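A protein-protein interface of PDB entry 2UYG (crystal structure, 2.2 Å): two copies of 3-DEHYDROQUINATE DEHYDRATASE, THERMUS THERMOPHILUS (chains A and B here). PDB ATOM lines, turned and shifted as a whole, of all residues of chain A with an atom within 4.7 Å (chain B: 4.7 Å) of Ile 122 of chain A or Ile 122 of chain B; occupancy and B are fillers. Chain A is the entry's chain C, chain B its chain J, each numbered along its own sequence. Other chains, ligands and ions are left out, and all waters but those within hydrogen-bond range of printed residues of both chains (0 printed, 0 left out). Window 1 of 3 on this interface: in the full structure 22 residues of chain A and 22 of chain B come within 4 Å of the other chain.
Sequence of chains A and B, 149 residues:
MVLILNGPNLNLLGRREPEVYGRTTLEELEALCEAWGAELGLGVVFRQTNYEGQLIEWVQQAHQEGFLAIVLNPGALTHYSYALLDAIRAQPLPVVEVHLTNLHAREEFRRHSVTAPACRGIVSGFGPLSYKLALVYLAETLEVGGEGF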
ATOM      1  N   GLU A  97      18.850   1.857  -6.283  1.00  0.00           N
ATOM      2  CA  GLU A  97      17.631   1.122  -6.611  1.00  0.00           C
ATOM      3  C   GLU A  97      17.469   0.924  -8.093  1.00  0.00           C
ATOM      4  O   GLU A  97      17.514   1.877  -8.850  1.00  0.00           O
ATOM      5  CB  GLU A  97      16.380   1.861  -6.085  1.00  0.00           C
ATOM      6  CG  GLU A  97      15.141   1.006  -6.208  1.00  0.00           C
ATOM      7  CD  GLU A  97      13.946   1.587  -5.442  1.00  0.00           C
ATOM      8  OE1 GLU A  97      12.851   1.756  -6.050  1.00  0.00           O
ATOM      9  OE2 GLU A  97      14.161   1.946  -4.290  1.00  0.00           O
ATOM     10  N   HIS A  99      15.272  -1.254 -11.350  1.00  0.00           N
ATOM     11  CA  HIS A  99      14.043  -1.991 -11.767  1.00  0.00           C
ATOM     12  C   HIS A  99      14.121  -2.219 -13.268  1.00  0.00           C
ATOM     13  O   HIS A  99      14.569  -1.340 -14.053  1.00  0.00           O
ATOM     14  CB  HIS A  99      12.761  -1.224 -11.516  1.00  0.00           C
ATOM     15  CG  HIS A  99      12.594  -0.782 -10.104  1.00  0.00           C
ATOM     16  ND1 HIS A  99      12.051  -1.600  -9.156  1.00  0.00           N
ATOM     17  CD2 HIS A  99      12.928   0.369  -9.472  1.00  0.00           C
ATOM     18  CE1 HIS A  99      12.059  -0.973  -7.999  1.00  0.00           C
ATOM     19  NE2 HIS A  99      12.571   0.229  -8.162  1.00  0.00           N
ATOM     20  N   HIS A 104       6.313   3.668 -13.843  1.00  0.00           N
ATOM     21  CA  HIS A 104       5.306   4.681 -14.129  1.00  0.00           C
ATOM     22  C   HIS A 104       4.393   4.402 -15.337  1.00  0.00           C
ATOM     23  O   HIS A 104       3.579   5.238 -15.673  1.00  0.00           O
ATOM     24  CB  HIS A 104       5.999   6.040 -14.235  1.00  0.00           C
ATOM     25  CG  HIS A 104       6.836   6.351 -13.033  1.00  0.00           C
ATOM     26  ND1 HIS A 104       8.203   6.351 -13.072  1.00  0.00           N
ATOM     27  CD2 HIS A 104       6.505   6.534 -11.731  1.00  0.00           C
ATOM     28  CE1 HIS A 104       8.688   6.633 -11.872  1.00  0.00           C
ATOM     29  NE2 HIS A 104       7.673   6.718 -11.035  1.00  0.00           N
ATOM     30  N   ALA A 116      13.052   4.031  -2.243  1.00  0.00           N
ATOM     31  CA  ALA A 116      13.814   5.037  -3.021  1.00  0.00           C
ATOM     32  C   ALA A 116      14.301   6.274  -2.266  1.00  0.00           C
ATOM     33  O   ALA A 116      15.342   6.748  -2.655  1.00  0.00           O
ATOM     34  CB  ALA A 116      13.113   5.450  -4.285  1.00  0.00           C
ATOM     35  N   GLY A 121      20.293   6.745  -5.716  1.00  0.00           N
ATOM     36  CA  GLY A 121      19.346   7.040  -6.774  1.00  0.00           C
ATOM     37  C   GLY A 121      18.682   5.795  -7.325  1.00  0.00           C
ATOM     38  O   GLY A 121      18.834   4.686  -6.832  1.00  0.00           O
ATOM     39  N   ILE A 122      17.960   6.002  -8.408  1.00  0.00           N
ATOM     40  CA  ILE A 122      17.059   5.012  -8.937  1.00  0.00           C
ATOM     41  C   ILE A 122      17.236   4.980 -10.465  1.00  0.00           C
ATOM     42  O   ILE A 122      17.312   6.013 -11.091  1.00  0.00           O
ATOM     43  CB  ILE A 122      15.627   5.307  -8.531  1.00  0.00           C
ATOM     44  CG1 ILE A 122      14.668   4.324  -9.216  1.00  0.00           C
ATOM     45  CG2 ILE A 122      15.233   6.736  -8.862  1.00  0.00           C
ATOM     46  CD1 ILE A 122      13.568   3.899  -8.379  1.00  0.00           C
ATOM     47  N   VAL A 123      17.396   3.781 -11.005  1.00  0.00           N
ATOM     48  CA  VAL A 123      17.277   3.611 -12.392  1.00  0.00           C
ATOM     49  C   VAL A 123      16.218   2.566 -12.762  1.00  0.00           C
ATOM     50  O   VAL A 123      16.222   1.403 -12.282  1.00  0.00           O
ATOM     51  CB  VAL A 123      18.666   3.374 -13.120  1.00  0.00           C
ATOM     52  CG1 VAL A 123      19.784   3.137 -12.211  1.00  0.00           C
ATOM     53  CG2 VAL A 123      18.536   2.342 -14.192  1.00  0.00           C
ATOM     54  N   SER A 124      15.350   2.959 -13.656  1.00  0.00           N
ATOM     55  CA  SER A 124      14.368   1.986 -14.125  1.00  0.00           C
ATOM     56  C   SER A 124      13.758   2.124 -15.501  1.00  0.00           C
ATOM     57  O   SER A 124      13.514   3.236 -16.029  1.00  0.00           O
ATOM     58  CB  SER A 124      13.259   1.896 -13.136  1.00  0.00           C
ATOM     59  OG  SER A 124      12.584   3.059 -13.215  1.00  0.00           O
ATOM     60  N   PHE A 126      14.947   0.020 -18.130  1.00  0.00           N
ATOM     61  CA  PHE A 126      15.901  -0.330 -19.188  1.00  0.00           C
ATOM     62  C   PHE A 126      16.140  -1.785 -19.361  1.00  0.00           C
ATOM     63  O   PHE A 126      17.082  -2.110 -20.001  1.00  0.00           O
ATOM     64  CB  PHE A 126      17.233   0.401 -18.901  1.00  0.00           C
ATOM     65  CG  PHE A 126      17.049   1.863 -18.723  1.00  0.00           C
ATOM     66  CD1 PHE A 126      17.128   2.444 -17.446  1.00  0.00           C
ATOM     67  CD2 PHE A 126      16.760   2.656 -19.821  1.00  0.00           C
ATOM     68  CE1 PHE A 126      16.980   3.766 -17.262  1.00  0.00           C
ATOM     69  CE2 PHE A 126      16.548   4.007 -19.659  1.00  0.00           C
ATOM     70  CZ  PHE A 126      16.642   4.577 -18.353  1.00  0.00           C
ATOM     71  N   GLU B  97      14.070   9.894 -19.318  1.00  0.00           N
ATOM     72  CA  GLU B  97      13.978  10.981 -18.363  1.00  0.00           C
ATOM     73  C   GLU B  97      15.127  10.906 -17.390  1.00  0.00           C
ATOM     74  O   GLU B  97      15.406   9.852 -16.901  1.00  0.00           O
ATOM     75  CB  GLU B  97      12.674  10.895 -17.584  1.00  0.00           C
ATOM     76  CG  GLU B  97      12.329  12.174 -16.881  1.00  0.00           C
ATOM     77  CD  GLU B  97      10.989  12.100 -16.191  1.00  0.00           C
ATOM     78  OE1 GLU B  97      10.994  12.342 -14.935  1.00  0.00           O
ATOM     79  OE2 GLU B  97       9.980  11.763 -16.878  1.00  0.00           O
ATOM     80  N   HIS B  99      17.186  13.087 -14.047  1.00  0.00           N
ATOM     81  CA  HIS B  99      17.251  14.143 -13.074  1.00  0.00           C
ATOM     82  C   HIS B  99      18.535  14.029 -12.313  1.00  0.00           C
ATOM     83  O   HIS B  99      19.080  12.929 -12.092  1.00  0.00           O
ATOM     84  CB  HIS B  99      16.114  14.052 -12.101  1.00  0.00           C
ATOM     85  CG  HIS B  99      14.763  13.992 -12.753  1.00  0.00           C
ATOM     86  ND1 HIS B  99      13.921  15.071 -12.807  1.00  0.00           N
ATOM     87  CD2 HIS B  99      14.146  13.024 -13.475  1.00  0.00           C
ATOM     88  CE1 HIS B  99      12.816  14.774 -13.475  1.00  0.00           C
ATOM     89  NE2 HIS B  99      12.918  13.525 -13.876  1.00  0.00           N
ATOM     90  N   HIS B 104      12.731  11.414  -4.590  1.00  0.00           N
ATOM     91  CA  HIS B 104      11.958  10.838  -3.516  1.00  0.00           C
ATOM     92  C   HIS B 104      12.502  11.185  -2.166  1.00  0.00           C
ATOM     93  O   HIS B 104      11.977  10.697  -1.193  1.00  0.00           O
ATOM     94  CB  HIS B 104      11.876   9.325  -3.667  1.00  0.00           C
ATOM     95  CG  HIS B 104      11.411   8.903  -5.014  1.00  0.00           C
ATOM     96  ND1 HIS B 104      12.254   8.351  -5.960  1.00  0.00           N
ATOM     97  CD2 HIS B 104      10.207   9.038  -5.616  1.00  0.00           C
ATOM     98  CE1 HIS B 104      11.577   8.123  -7.069  1.00  0.00           C
ATOM     99  NE2 HIS B 104      10.341   8.549  -6.893  1.00  0.00           N
ATOM    100  N   ALA B 116       7.193  10.672 -17.048  1.00  0.00           N
ATOM    101  CA  ALA B 116       7.686   9.317 -16.882  1.00  0.00           C
ATOM    102  C   ALA B 116       6.898   8.170 -17.572  1.00  0.00           C
ATOM    103  O   ALA B 116       7.504   7.231 -18.146  1.00  0.00           O
ATOM    104  CB  ALA B 116       7.896   9.028 -15.322  1.00  0.00           C
ATOM    105  N   GLY B 121      12.533   4.995 -19.847  1.00  0.00           N
ATOM    106  CA  GLY B 121      12.945   4.756 -18.473  1.00  0.00           C
ATOM    107  C   GLY B 121      13.351   6.039 -17.866  1.00  0.00           C
ATOM    108  O   GLY B 121      13.248   7.062 -18.536  1.00  0.00           O
ATOM    109  N   ILE B 122      13.849   5.991 -16.637  1.00  0.00           N
ATOM    110  CA  ILE B 122      14.120   7.168 -15.860  1.00  0.00           C
ATOM    111  C   ILE B 122      15.313   6.926 -15.010  1.00  0.00           C
ATOM    112  O   ILE B 122      15.463   5.829 -14.462  1.00  0.00           O
ATOM    113  CB  ILE B 122      12.891   7.558 -14.952  1.00  0.00           C
ATOM    114  CG1 ILE B 122      13.253   8.734 -14.052  1.00  0.00           C
ATOM    115  CG2 ILE B 122      12.470   6.342 -14.070  1.00  0.00           C
ATOM    116  CD1 ILE B 122      12.090   9.668 -13.692  1.00  0.00           C
ATOM    117  N   VAL B 123      16.206   7.920 -14.923  1.00  0.00           N
ATOM    118  CA  VAL B 123      17.292   7.746 -14.064  1.00  0.00           C
ATOM    119  C   VAL B 123      17.413   9.021 -13.308  1.00  0.00           C
ATOM    120  O   VAL B 123      17.224  10.127 -13.867  1.00  0.00           O
ATOM    121  CB  VAL B 123      18.608   7.185 -14.791  1.00  0.00           C
ATOM    122  CG1 VAL B 123      18.447   7.015 -16.246  1.00  0.00           C
ATOM    123  CG2 VAL B 123      19.884   7.927 -14.402  1.00  0.00           C
ATOM    124  N   SER B 124      17.659   8.886 -11.994  1.00  0.00           N
ATOM    125  CA  SER B 124      17.576  10.065 -11.195  1.00  0.00           C
ATOM    126  C   SER B 124      18.373   9.994  -9.906  1.00  0.00           C
ATOM    127  O   SER B 124      18.453   8.933  -9.282  1.00  0.00           O
ATOM    128  CB  SER B 124      16.085  10.394 -11.052  1.00  0.00           C
ATOM    129  OG  SER B 124      15.649   9.961  -9.852  1.00  0.00           O
ATOM    130  N   PHE B 126      21.796  10.859  -9.577  1.00  0.00           N
ATOM    131  CA  PHE B 126      23.253  10.703  -9.753  1.00  0.00           C
ATOM    132  C   PHE B 126      24.067  11.979 -10.120  1.00  0.00           C
ATOM    133  O   PHE B 126      25.181  11.897 -10.587  1.00  0.00           O
ATOM    134  CB  PHE B 126      23.485   9.575 -10.722  1.00  0.00           C
ATOM    135  CG  PHE B 126      22.797   8.314 -10.311  1.00  0.00           C
ATOM    136  CD1 PHE B 126      21.563   7.968 -10.854  1.00  0.00           C
ATOM    137  CD2 PHE B 126      23.344   7.497  -9.346  1.00  0.00           C
ATOM    138  CE1 PHE B 126      20.924   6.846 -10.470  1.00  0.00           C
ATOM    139  CE2 PHE B 126      22.705   6.339  -8.989  1.00  0.00           C
ATOM    140  CZ  PHE B 126      21.466   6.041  -9.540  1.00  0.00           C
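O of Ile 122 of chain A sits at hydrogen-bond distance from N of Ser 124 of chain B (3.0 Å).
O of Ser 124 of chain A is in hydrogen-bond range of N of Ile 122 of chain B, 2.8 Å away.
The backbone NH of Ala 116 of chain A sits at hydrogen-bond distance from the side-chain carboxylate of Glu 97 of chain A (3.1 Å).
The backbone NH of Glu 97 of chain A lies within hydrogen-bond range of the backbone carbonyl oxygen of Gly 121 of chain A (2.9 Å).
O of Glu 97 of chain A lies within hydrogen-bond range of N of Val 123 of chain A (2.9 Å).
N of Ala 116 of chain B lies within hydrogen-bond range of OE2 of Glu 97 of chain B, 3.0 Å away.
N of Val 123 of chain B lies within hydrogen-bond range of O of Glu 97 of chain B (2.9 Å).
O of Val 123 of chain B is in hydrogen-bond range of N of His 99 of chain B.
ND1 of His 104 of chain A touches CB of Ala 116 of chain B, at 3.5 Å.
ND1 of His 104 of chain B touches CB of Ala 116 of chain A, at 3.5 Å.
Gly 121 of chain A touches Ser 124 of chain B (CA to O, 3.3 Å).
C of Gly 121 of chain A touches CZ of Phe 126 of chain B (3.6 Å).
Ile 122 of chain B touches Ile 122 of chain A (O to O, 3.8 Å).
Val 123 of chain A touches Ile 122 of chain B.
Ser 124 of chain A touches Gly 121 of chain B (O to CA, 2.9 Å).
Phe 126 of chain A touches Gly 121 of chain B.
CZ of Phe 126 of chain A touches N of Ile 122 of chain B, 3.6 Å away.
Val 123 of chain B touches Phe 126 of chain A (CG1 to CZ, 3.7 Å).
Of chain B, only Ile 122, Val 123, Ser 124 and Phe 126 come within 4 Å of Ile 122 of chain A.
Of the printed residues of chain A, Ala 116 of chain B touches His 104 (3.5 Å).
Ile 122 of chain B touches just these residues of chain A: Ile 122 (3.8 Å), Val 123 (3.5 Å), Ser 124 (2.8 Å) and Phe 126 (3.6 Å).
Of the printed residues of chain A, Val 123 of chain B touches Ile 122 and Phe 126.
The nearest residue of chain B that does not touch Ile 122 of chain A is His 104 of chain B (4.3 Å).
Printed residues of chain A that touch a printed residue of chain B: His 104, Ala 116, Gly 121, Ile 122, Val 123, Ser 124 and Phe 126.
Hydrophobic or aromatic side chains of chain A within 4 Å of the printed part of chain B: His 104, Ala 116, Ile 122 and Phe 126.
Along chain A the printed residues that touch a printed residue of chain B span positions 104 to 126.
Of the 9 printed residues of chain B, 7 touch a printed residue of chain A.
Hydrophobic or aromatic side chains of chain B within 4 Å of the printed part of chain A: His 104, Ala 116, Ile 122, Val 123 and Phe 126.
Among the printed residues, no Asp or Glu carboxylate lies within 4 Å of a Lys or Arg side-chain nitrogen of the other chain.
His 104 of chain A touches Ala 116 of chain B, and with the chains exchanged Ala 116 of chain A touches His 104 of chain B.
Ile 122 of chain A touches its own counterpart, Ile 122 of chain B.
Ile 122 of chain A touches Val 123 of chain B, and with the chains exchanged Val 123 of chain A touches Ile 122 of chain B.
Ile 122 of chain A touches Ser 124 of chain B, and with the chains exchanged Ser 124 of chain A touches Ile 122 of chain B.
Of the 14 pairs that touch across the chains among the printed residues, 13 have their exchanged pair printed and touching as well.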
